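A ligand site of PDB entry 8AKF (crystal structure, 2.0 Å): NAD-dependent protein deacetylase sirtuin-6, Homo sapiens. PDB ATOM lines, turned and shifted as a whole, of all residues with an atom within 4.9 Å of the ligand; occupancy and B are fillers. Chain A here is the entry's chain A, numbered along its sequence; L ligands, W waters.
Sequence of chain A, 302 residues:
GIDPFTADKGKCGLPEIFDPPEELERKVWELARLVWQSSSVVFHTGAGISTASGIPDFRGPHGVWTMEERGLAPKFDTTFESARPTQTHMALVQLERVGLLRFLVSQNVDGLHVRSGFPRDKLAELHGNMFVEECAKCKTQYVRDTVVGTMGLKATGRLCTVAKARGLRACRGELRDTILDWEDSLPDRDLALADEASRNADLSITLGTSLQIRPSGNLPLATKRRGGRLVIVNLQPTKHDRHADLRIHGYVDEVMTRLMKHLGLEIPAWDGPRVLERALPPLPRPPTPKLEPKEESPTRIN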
ATOM      1  N   GLU A  16      27.962   8.032 -27.672  1.00  0.00           N
ATOM      2  CA  GLU A  16      28.761   9.174 -28.139  1.00  0.00           C
ATOM      3  C   GLU A  16      29.368   8.806 -29.497  1.00  0.00           C
ATOM      4  O   GLU A  16      29.761   7.629 -29.692  1.00  0.00           O
ATOM      5  CB  GLU A  16      29.752   9.552 -27.060  1.00  0.00           C
ATOM      6  CG  GLU A  16      29.007  10.125 -25.856  1.00  0.00           C
ATOM      7  CD  GLU A  16      29.904  10.785 -24.853  1.00  0.00           C
ATOM      8  OE1 GLU A  16      31.050  10.347 -24.717  1.00  0.00           O
ATOM      9  OE2 GLU A  16      29.459  11.749 -24.232  1.00  0.00           O
ATOM     10  N   GLY A  46      22.468  24.307 -24.796  1.00  0.00           N
ATOM     11  CA  GLY A  46      21.873  23.290 -23.925  1.00  0.00           C
ATOM     12  C   GLY A  46      23.010  22.745 -23.059  1.00  0.00           C
ATOM     13  O   GLY A  46      24.163  23.262 -23.250  1.00  0.00           O
ATOM     14  N   ALA A  47      22.708  21.781 -22.219  1.00  0.00           N
ATOM     15  CA  ALA A  47      23.378  21.444 -20.935  1.00  0.00           C
ATOM     16  C   ALA A  47      24.772  20.914 -21.218  1.00  0.00           C
ATOM     17  O   ALA A  47      25.573  20.942 -20.286  1.00  0.00           O
ATOM     18  CB  ALA A  47      22.587  20.437 -20.114  1.00  0.00           C
ATOM     19  N   GLY A  48      25.040  20.523 -22.466  1.00  0.00           N
ATOM     20  CA  GLY A  48      26.312  19.909 -22.873  1.00  0.00           C
ATOM     21  C   GLY A  48      27.453  20.915 -22.828  1.00  0.00           C
ATOM     22  O   GLY A  48      28.577  20.475 -22.536  1.00  0.00           O
ATOM     23  N   THR A  51      28.987  20.880 -19.057  1.00  0.00           N
ATOM     24  CA  THR A  51      29.505  19.602 -18.502  1.00  0.00           C
ATOM     25  C   THR A  51      30.971  19.781 -18.123  1.00  0.00           C
ATOM     26  O   THR A  51      31.356  19.167 -17.125  1.00  0.00           O
ATOM     27  CB  THR A  51      29.276  18.379 -19.411  1.00  0.00           C
ATOM     28  OG1 THR A  51      29.688  18.685 -20.743  1.00  0.00           O
ATOM     29  CG2 THR A  51      27.858  17.815 -19.329  1.00  0.00           C
ATOM     30  N   ASP A  57      24.807  16.893 -17.627  1.00  0.00           N
ATOM     31  CA  ASP A  57      23.689  17.154 -18.569  1.00  0.00           C
ATOM     32  C   ASP A  57      22.484  16.289 -18.191  1.00  0.00           C
ATOM     33  O   ASP A  57      22.503  15.640 -17.139  1.00  0.00           O
ATOM     34  CB  ASP A  57      24.138  17.003 -20.027  1.00  0.00           C
ATOM     35  CG  ASP A  57      24.681  15.642 -20.452  1.00  0.00           C
ATOM     36  OD1 ASP A  57      24.482  14.650 -19.742  1.00  0.00           O
ATOM     37  OD2 ASP A  57      25.304  15.601 -21.530  1.00  0.00           O
ATOM     38  N   PHE A  58      21.450  16.311 -19.023  1.00  0.00           N
ATOM     39  CA  PHE A  58      20.227  15.499 -18.795  1.00  0.00           C
ATOM     40  C   PHE A  58      20.300  14.148 -19.501  1.00  0.00           C
ATOM     41  O   PHE A  58      19.995  13.157 -18.816  1.00  0.00           O
ATOM     42  CB  PHE A  58      18.986  16.312 -19.157  1.00  0.00           C
ATOM     43  CG  PHE A  58      18.821  17.594 -18.360  1.00  0.00           C
ATOM     44  CD1 PHE A  58      18.205  17.569 -17.120  1.00  0.00           C
ATOM     45  CD2 PHE A  58      19.282  18.805 -18.842  1.00  0.00           C
ATOM     46  CE1 PHE A  58      18.052  18.740 -16.379  1.00  0.00           C
ATOM     47  CE2 PHE A  58      19.138  19.972 -18.097  1.00  0.00           C
ATOM     48  CZ  PHE A  58      18.501  19.936 -16.873  1.00  0.00           C
ATOM     49  N   ARG A  59      20.661  14.072 -20.790  1.00  0.00           N
ATOM     50  CA  ARG A  59      20.505  12.793 -21.519  1.00  0.00           C
ATOM     51  C   ARG A  59      21.841  12.226 -22.029  1.00  0.00           C
ATOM     52  O   ARG A  59      21.800  11.234 -22.821  1.00  0.00           O
ATOM     53  CB  ARG A  59      19.493  12.982 -22.642  1.00  0.00           C
ATOM     54  CG  ARG A  59      18.250  13.694 -22.124  1.00  0.00           C
ATOM     55  CD  ARG A  59      17.256  13.861 -23.256  1.00  0.00           C
ATOM     56  NE  ARG A  59      16.086  14.508 -22.754  1.00  0.00           N
ATOM     57  CZ  ARG A  59      15.988  15.779 -22.368  1.00  0.00           C
ATOM     58  NH1 ARG A  59      16.981  16.634 -22.534  1.00  0.00           N
ATOM     59  NH2 ARG A  59      14.815  16.220 -21.952  1.00  0.00           N
ATOM     60  N   GLY A  60      22.965  12.755 -21.545  1.00  0.00           N
ATOM     61  CA  GLY A  60      24.328  12.224 -21.810  1.00  0.00           C
ATOM     62  C   GLY A  60      24.562  10.938 -21.013  1.00  0.00           C
ATOM     63  O   GLY A  60      23.809  10.652 -20.088  1.00  0.00           O
ATOM     64  N   TRP A  65      18.637  12.596 -16.297  1.00  0.00           N
ATOM     65  CA  TRP A  65      17.588  11.667 -16.806  1.00  0.00           C
ATOM     66  C   TRP A  65      18.174  10.273 -17.036  1.00  0.00           C
ATOM     67  O   TRP A  65      17.509   9.289 -16.702  1.00  0.00           O
ATOM     68  CB  TRP A  65      16.956  12.201 -18.095  1.00  0.00           C
ATOM     69  CG  TRP A  65      16.249  13.520 -18.008  1.00  0.00           C
ATOM     70  CD1 TRP A  65      15.934  14.294 -19.092  1.00  0.00           C
ATOM     71  CD2 TRP A  65      15.725  14.204 -16.855  1.00  0.00           C
ATOM     72  NE1 TRP A  65      15.274  15.417 -18.684  1.00  0.00           N
ATOM     73  CE2 TRP A  65      15.135  15.400 -17.323  1.00  0.00           C
ATOM     74  CE3 TRP A  65      15.682  13.933 -15.478  1.00  0.00           C
ATOM     75  CZ2 TRP A  65      14.525  16.316 -16.476  1.00  0.00           C
ATOM     76  CZ3 TRP A  65      15.085  14.848 -14.636  1.00  0.00           C
ATOM     77  CH2 TRP A  65      14.518  16.024 -15.121  1.00  0.00           C
ATOM     78  N   GLN A 107      18.558  26.909 -23.449  1.00  0.00           N
ATOM     79  CA  GLN A 107      17.708  26.024 -22.643  1.00  0.00           C
ATOM     80  C   GLN A 107      18.228  26.026 -21.220  1.00  0.00           C
ATOM     81  O   GLN A 107      17.537  25.545 -20.388  1.00  0.00           O
ATOM     82  CB  GLN A 107      17.724  24.708 -23.371  1.00  0.00           C
ATOM     83  CG  GLN A 107      16.716  24.715 -24.494  1.00  0.00           C
ATOM     84  CD  GLN A 107      16.830  23.489 -25.362  1.00  0.00           C
ATOM     85  OE1 GLN A 107      16.098  22.538 -25.163  1.00  0.00           O
ATOM     86  NE2 GLN A 107      17.773  23.491 -26.299  1.00  0.00           N
ATOM     87  N   ASN A 108      19.457  26.532 -20.948  1.00  0.00           N
ATOM     88  CA  ASN A 108      20.119  26.262 -19.634  1.00  0.00           C
ATOM     89  C   ASN A 108      19.615  27.224 -18.553  1.00  0.00           C
ATOM     90  O   ASN A 108      19.522  28.404 -18.835  1.00  0.00           O
ATOM     91  CB  ASN A 108      21.628  26.313 -19.697  1.00  0.00           C
ATOM     92  CG  ASN A 108      22.153  25.386 -20.765  1.00  0.00           C
ATOM     93  OD1 ASN A 108      21.668  24.286 -20.959  1.00  0.00           O
ATOM     94  ND2 ASN A 108      23.113  25.846 -21.510  1.00  0.00           N
ATOM     95  N   HIS A 127      14.086  28.254 -20.596  1.00  0.00           N
ATOM     96  CA  HIS A 127      13.626  27.481 -19.418  1.00  0.00           C
ATOM     97  C   HIS A 127      13.852  28.285 -18.126  1.00  0.00           C
ATOM     98  O   HIS A 127      13.516  27.751 -17.059  1.00  0.00           O
ATOM     99  CB  HIS A 127      14.258  26.071 -19.447  1.00  0.00           C
ATOM    100  CG  HIS A 127      14.073  25.336 -20.739  1.00  0.00           C
ATOM    101  ND1 HIS A 127      14.899  24.270 -21.151  1.00  0.00           N
ATOM    102  CD2 HIS A 127      13.169  25.537 -21.723  1.00  0.00           C
ATOM    103  CE1 HIS A 127      14.489  23.842 -22.297  1.00  0.00           C
ATOM    104  NE2 HIS A 127      13.420  24.652 -22.682  1.00  0.00           N
ATOM    105  N   TRP A 182       7.421  21.061 -15.783  1.00  0.00           N
ATOM    106  CA  TRP A 182       6.974  20.296 -16.984  1.00  0.00           C
ATOM    107  C   TRP A 182       5.765  20.986 -17.648  1.00  0.00           C
ATOM    108  O   TRP A 182       5.762  21.043 -18.885  1.00  0.00           O
ATOM    109  CB  TRP A 182       6.677  18.847 -16.575  1.00  0.00           C
ATOM    110  CG  TRP A 182       7.911  18.070 -16.216  1.00  0.00           C
ATOM    111  CD1 TRP A 182       8.353  17.741 -14.964  1.00  0.00           C
ATOM    112  CD2 TRP A 182       8.892  17.547 -17.133  1.00  0.00           C
ATOM    113  NE1 TRP A 182       9.535  17.042 -15.031  1.00  0.00           N
ATOM    114  CE2 TRP A 182       9.900  16.921 -16.346  1.00  0.00           C
ATOM    115  CE3 TRP A 182       9.037  17.552 -18.520  1.00  0.00           C
ATOM    116  CZ2 TRP A 182      11.010  16.308 -16.919  1.00  0.00           C
ATOM    117  CZ3 TRP A 182      10.134  16.941 -19.088  1.00  0.00           C
ATOM    118  CH2 TRP A 182      11.108  16.328 -18.291  1.00  0.00           C
ATOM    119  N   GLY A 208      26.061  21.487 -27.705  1.00  0.00           N
ATOM    120  CA  GLY A 208      25.771  20.652 -26.523  1.00  0.00           C
ATOM    121  C   GLY A 208      24.284  20.561 -26.172  1.00  0.00           C
ATOM    122  O   GLY A 208      24.000  20.561 -24.973  1.00  0.00           O
ATOM    123  N   THR A 209      23.375  20.502 -27.153  1.00  0.00           N
ATOM    124  CA  THR A 209      21.907  20.219 -26.978  1.00  0.00           C
ATOM    125  C   THR A 209      21.475  18.998 -27.822  1.00  0.00           C
ATOM    126  O   THR A 209      22.043  18.791 -28.881  1.00  0.00           O
ATOM    127  CB  THR A 209      21.043  21.432 -27.309  1.00  0.00           C
ATOM    128  OG1 THR A 209      19.664  21.054 -27.189  1.00  0.00           O
ATOM    129  CG2 THR A 209      21.296  21.983 -28.684  1.00  0.00           C
ATOM    130  N   SER A 210      20.472  18.238 -27.376  1.00  0.00           N
ATOM    131  CA  SER A 210      19.950  17.070 -28.121  1.00  0.00           C
ATOM    132  C   SER A 210      18.685  17.455 -28.900  1.00  0.00           C
ATOM    133  O   SER A 210      18.314  16.650 -29.721  1.00  0.00           O
ATOM    134  CB  SER A 210      19.766  15.823 -27.262  1.00  0.00           C
ATOM    135  OG  SER A 210      18.934  16.025 -26.165  1.00  0.00           O
ATOM    136  N   LEU A 211      18.158  18.673 -28.708  1.00  0.00           N
ATOM    137  CA  LEU A 211      17.104  19.310 -29.567  1.00  0.00           C
ATOM    138  C   LEU A 211      15.792  18.521 -29.490  1.00  0.00           C
ATOM    139  O   LEU A 211      14.959  18.566 -30.439  1.00  0.00           O
ATOM    140  CB  LEU A 211      17.627  19.438 -31.005  1.00  0.00           C
ATOM    141  CG  LEU A 211      18.965  20.148 -31.166  1.00  0.00           C
ATOM    142  CD1 LEU A 211      19.417  20.127 -32.613  1.00  0.00           C
ATOM    143  CD2 LEU A 211      18.896  21.581 -30.659  1.00  0.00           C
ATOM    144  N   ILE A 213      13.395  18.828 -26.993  1.00  0.00           N
ATOM    145  CA  ILE A 213      12.336  19.540 -26.224  1.00  0.00           C
ATOM    146  C   ILE A 213      11.735  20.573 -27.177  1.00  0.00           C
ATOM    147  O   ILE A 213      12.519  21.320 -27.803  1.00  0.00           O
ATOM    148  CB  ILE A 213      12.896  20.161 -24.911  1.00  0.00           C
ATOM    149  CG1 ILE A 213      13.332  19.070 -23.929  1.00  0.00           C
ATOM    150  CG2 ILE A 213      11.903  21.121 -24.270  1.00  0.00           C
ATOM    151  CD1 ILE A 213      12.196  18.219 -23.374  1.00  0.00           C
ATOM    152  N   VAL A 233      26.604  20.942 -33.204  1.00  0.00           N
ATOM    153  CA  VAL A 233      27.786  20.456 -32.412  1.00  0.00           C
ATOM    154  C   VAL A 233      27.300  19.645 -31.214  1.00  0.00           C
ATOM    155  O   VAL A 233      26.623  20.190 -30.221  1.00  0.00           O
ATOM    156  CB  VAL A 233      28.747  21.608 -31.998  1.00  0.00           C
ATOM    157  CG1 VAL A 233      30.008  21.065 -31.337  1.00  0.00           C
ATOM    158  CG2 VAL A 233      29.145  22.500 -33.158  1.00  0.00           C
ATOM    159  N   ASN A 234      27.551  18.337 -31.235  1.00  0.00           N
ATOM    160  CA  ASN A 234      27.033  17.457 -30.164  1.00  0.00           C
ATOM    161  C   ASN A 234      27.752  16.117 -30.190  1.00  0.00           C
ATOM    162  O   ASN A 234      28.052  15.600 -31.282  1.00  0.00           O
ATOM    163  CB  ASN A 234      25.517  17.264 -30.275  1.00  0.00           C
ATOM    164  CG  ASN A 234      24.852  17.089 -28.935  1.00  0.00           C
ATOM    165  OD1 ASN A 234      24.727  18.049 -28.166  1.00  0.00           O
ATOM    166  ND2 ASN A 234      24.355  15.899 -28.647  1.00  0.00           N
ATOM    167  N   LEU A 235      28.020  15.586 -29.001  1.00  0.00           N
ATOM    168  CA  LEU A 235      28.700  14.267 -28.862  1.00  0.00           C
ATOM    169  C   LEU A 235      27.755  13.123 -29.252  1.00  0.00           C
ATOM    170  O   LEU A 235      28.242  12.142 -29.879  1.00  0.00           O
ATOM    171  CB  LEU A 235      29.177  14.141 -27.412  1.00  0.00           C
ATOM    172  CG  LEU A 235      30.540  14.751 -27.159  1.00  0.00           C
ATOM    173  CD1 LEU A 235      30.825  14.802 -25.685  1.00  0.00           C
ATOM    174  CD2 LEU A 235      31.628  13.974 -27.922  1.00  0.00           C
ATOM    175  N   GLN A 236      26.473  13.247 -28.949  1.00  0.00           N
ATOM    176  CA  GLN A 236      25.405  12.232 -29.172  1.00  0.00           C
ATOM    177  C   GLN A 236      24.581  12.715 -30.362  1.00  0.00           C
ATOM    178  O   GLN A 236      24.676  13.895 -30.728  1.00  0.00           O
ATOM    179  CB  GLN A 236      24.475  12.120 -27.964  1.00  0.00           C
ATOM    180  CG  GLN A 236      25.030  11.381 -26.753  1.00  0.00           C
ATOM    181  CD  GLN A 236      24.002  11.326 -25.642  1.00  0.00           C
ATOM    182  OE1 GLN A 236      23.259  12.276 -25.427  1.00  0.00           O
ATOM    183  NE2 GLN A 236      23.933  10.211 -24.948  1.00  0.00           N
ATOM    184  N   PRO A 237      23.815  11.823 -31.031  1.00  0.00           N
ATOM    185  CA  PRO A 237      22.800  12.244 -32.002  1.00  0.00           C
ATOM    186  C   PRO A 237      21.758  13.197 -31.416  1.00  0.00           C
ATOM    187  O   PRO A 237      21.593  13.158 -30.259  1.00  0.00           O
ATOM    188  CB  PRO A 237      22.133  10.921 -32.426  1.00  0.00           C
ATOM    189  CG  PRO A 237      23.215   9.884 -32.186  1.00  0.00           C
ATOM    190  CD  PRO A 237      23.980  10.361 -30.974  1.00  0.00           C
ATOM    191  N   GLY A 250      32.207  16.044 -31.246  1.00  0.00           N
ATOM    192  CA  GLY A 250      33.418  16.424 -30.486  1.00  0.00           C
ATOM    193  C   GLY A 250      33.041  17.274 -29.298  1.00  0.00           C
ATOM    194  O   GLY A 250      31.848  17.663 -29.237  1.00  0.00           O
ATOM    195  N   TYR A 251      33.988  17.507 -28.367  1.00  0.00           N
ATOM    196  CA  TYR A 251      33.795  18.357 -27.169  1.00  0.00           C
ATOM    197  C   TYR A 251      33.652  19.806 -27.640  1.00  0.00           C
ATOM    198  O   TYR A 251      34.445  20.328 -28.508  1.00  0.00           O
ATOM    199  CB  TYR A 251      34.910  18.203 -26.143  1.00  0.00           C
ATOM    200  CG  TYR A 251      35.027  16.808 -25.585  1.00  0.00           C
ATOM    201  CD1 TYR A 251      34.164  16.349 -24.602  1.00  0.00           C
ATOM    202  CD2 TYR A 251      35.999  15.942 -26.060  1.00  0.00           C
ATOM    203  CE1 TYR A 251      34.282  15.060 -24.078  1.00  0.00           C
ATOM    204  CE2 TYR A 251      36.125  14.650 -25.556  1.00  0.00           C
ATOM    205  CZ  TYR A 251      35.255  14.204 -24.573  1.00  0.00           C
ATOM    206  OH  TYR A 251      35.396  12.944 -24.074  1.00  0.00           O
ATOM    207  N   VAL A 252      32.612  20.443 -27.127  1.00  0.00           N
ATOM    208  CA  VAL A 252      32.264  21.785 -27.633  1.00  0.00           C
ATOM    209  C   VAL A 252      33.409  22.748 -27.287  1.00  0.00           C
ATOM    210  O   VAL A 252      33.787  23.545 -28.142  1.00  0.00           O
ATOM    211  CB  VAL A 252      30.885  22.259 -27.168  1.00  0.00           C
ATOM    212  CG1 VAL A 252      30.837  22.532 -25.652  1.00  0.00           C
ATOM    213  CG2 VAL A 252      30.485  23.465 -27.957  1.00  0.00           C
HETATM  214  N1  LIG L   1      30.698  18.640 -25.942  1.00  0.00           N
HETATM  215  C1  LIG L   1      29.745  18.346 -26.837  1.00  0.00           C
HETATM  216  N2  LIG L   1      28.555  17.778 -26.637  1.00  0.00           N
HETATM  217  C2  LIG L   1      28.348  17.566 -25.335  1.00  0.00           C
HETATM  218  C3  LIG L   1      29.226  17.822 -24.303  1.00  0.00           C
HETATM  219  C4  LIG L   1      30.470  18.393 -24.627  1.00  0.00           C
HETATM  220  N3  LIG L   1      31.424  18.721 -23.757  1.00  0.00           N
HETATM  221  N4  LIG L   1      28.653  17.445 -23.101  1.00  0.00           N
HETATM  222  C5  LIG L   1      27.450  17.035 -23.421  1.00  0.00           C
HETATM  223  N5  LIG L   1      27.236  17.040 -24.762  1.00  0.00           N
HETATM  224  P1  LIG L   1      20.502  17.130 -23.172  1.00  0.00           P
HETATM  225  P2  LIG L   1      19.366  19.819 -23.375  1.00  0.00           P
HETATM  226  C6  LIG L   1      26.020  16.623 -25.465  1.00  0.00           C
HETATM  227  O1  LIG L   1      19.239  16.562 -23.750  1.00  0.00           O
HETATM  228  O2  LIG L   1      19.883  21.162 -23.019  1.00  0.00           O
HETATM  229  C7  LIG L   1      15.628  19.048 -19.773  1.00  0.00           C
HETATM  230  O3  LIG L   1      14.515  18.411 -19.251  1.00  0.00           O
HETATM  231  C8  LIG L   1      25.397  15.281 -25.062  1.00  0.00           C
HETATM  232  O4  LIG L   1      25.812  14.298 -25.985  1.00  0.00           O
HETATM  233  O5  LIG L   1      21.131  16.345 -22.067  1.00  0.00           O
HETATM  234  O6  LIG L   1      19.333  19.443 -24.804  1.00  0.00           O
HETATM  235  C9  LIG L   1      15.765  20.540 -19.415  1.00  0.00           C
HETATM  236  O7  LIG L   1      14.542  21.267 -19.363  1.00  0.00           O
HETATM  237  C10 LIG L   1      23.884  15.548 -25.193  1.00  0.00           C
HETATM  238  O8  LIG L   1      23.442  15.042 -26.421  1.00  0.00           O
HETATM  239  O9  LIG L   1      20.256  18.661 -22.672  1.00  0.00           O
HETATM  240  C11 LIG L   1      16.649  21.049 -20.560  1.00  0.00           C
HETATM  241  O10 LIG L   1      16.634  22.472 -20.677  1.00  0.00           O
HETATM  242  C12 LIG L   1      23.735  17.070 -25.171  1.00  0.00           C
HETATM  243  O11 LIG L   1      25.085  17.610 -25.120  1.00  0.00           O
HETATM  244  C13 LIG L   1      15.972  20.312 -21.716  1.00  0.00           C
HETATM  245  O12 LIG L   1      15.585  19.026 -21.181  1.00  0.00           O
HETATM  246  C14 LIG L   1      22.939  17.660 -24.051  1.00  0.00           C
HETATM  247  O13 LIG L   1      21.530  17.442 -24.326  1.00  0.00           O
HETATM  248  C15 LIG L   1      16.780  20.111 -22.971  1.00  0.00           C
HETATM  249  O14 LIG L   1      18.013  19.446 -22.635  1.00  0.00           O
HETATM  250  O   HOH W   1      21.098  12.677 -26.875  1.00  0.00           O
HETATM  251  O   HOH W   2      19.298  22.640 -20.731  1.00  0.00           O
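The backbone carbonyl oxygen (O) of Gly 48 sits close to a nitrogen (N4) of the ligand. O11 of the ligand lies close to O of Gly 208, 3.1 Å away. Residues that only touch the ligand: Gly 46 (3.1 Å), Asp 57 (3.2 Å), Gly 250 (3.3 Å), Tyr 251 (3.3 Å) and Ile 213 (3.6 Å). Hydrophobic or aromatic side chains within 4 Å of the ligand: Ala 47, Phe 58, Trp 65, His 127, Ile 213, Leu 235, Tyr 251 and Val 252. Along chain A the residues within 4 Å of the ligand span positions 46 to 252. The nearest printed residue that does not touch the ligand is Gly 60 (4.1 Å).
O of Phe 58 is in hydrogen-bond range of N of Trp 65 (2.9 Å). The side-chain hydroxyl of Thr 51 sits at hydrogen-bond distance from the backbone carbonyl oxygen of Gly 48, 2.8 Å away. O of Gln 236 is in hydrogen-bond range of ND2 of Asn 234 (2.9 Å). The backbone carbonyl oxygen of Gln 107 lies within hydrogen-bond range of a ring nitrogen (ND1) of His 127, at 3.0 Å. N of Gly 48 lies within hydrogen-bond range of O of Gly 208 (2.7 Å). N of Gly 60 is in hydrogen-bond range of OD1 of Asp 57, at 3.0 Å. The side-chain amide nitrogen (NE2) of Gln 107 is in hydrogen-bond range of the side-chain hydroxyl (OG1) of Thr 209, 3.2 Å away. The backbone NH (N) of Ala 47 is in hydrogen-bond range of the backbone carbonyl oxygen (O) of Gly 208, 3.3 Å away.
Water W2 lies within hydrogen-bond range of an oxygen (O10) of the ligand, the side-chain amide oxygen (OD1) of Asn 108 and the backbone carbonyl oxygen (O) of Gln 107. Water W1 lies within hydrogen-bond range of OE1 of Gln 236 (2.6 Å), O8 of the ligand (3.4 Å) and O of Pro 237 (3.5 Å).
OG1 of Thr 209 is in hydrogen-bond range of O6 of the ligand (2.9 Å). The backbone carbonyl oxygen of Gln 107 sits at hydrogen-bond distance from an oxygen (O10) of the ligand (3.2 Å). The backbone NH of Gln 236 sits close to an oxygen (O4) of the ligand (3.2 Å). An oxygen (O3) of the ligand lies within hydrogen-bond range of the indole nitrogen of Trp 65, at 3.1 Å. An oxygen (O8) of the ligand sits at hydrogen-bond distance from the side-chain amide nitrogen (ND2) of Asn 234, at 2.6 Å. The guanidinium group (NH1) of Arg 59 is in salt-bridge range of an oxygen (O1) of the ligand, at 2.6 Å. The backbone NH (N) of Leu 235 sits at hydrogen-bond distance from a nitrogen (N2) of the ligand (3.3 Å). An oxygen (O6) of the ligand is in hydrogen-bond range of the backbone NH (N) of Ser 210, at 3.1 Å. The side-chain hydroxyl (OG1) of Thr 51 is in hydrogen-bond range of a nitrogen (N4) of the ligand (2.9 Å). The side-chain amide oxygen of Gln 236 sits at hydrogen-bond distance from an oxygen (O8) of the ligand, at 2.9 Å. The backbone NH of Ala 47 sits at hydrogen-bond distance from an oxygen (O2) of the ligand (3.0 Å). N of Arg 59 sits at hydrogen-bond distance from O5 of the ligand. An oxygen (O10) of the ligand sits at hydrogen-bond distance from a ring nitrogen (ND1) of His 127 (2.5 Å). O1 of the ligand lies within hydrogen-bond range of OG of Ser 210 (2.5 Å). An oxygen (O5) of the ligand lies within hydrogen-bond range of the backbone NH (N) of Phe 58, at 3.1 Å. N of Val 252 is in hydrogen-bond range of N1 of the ligand, 2.9 Å away.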
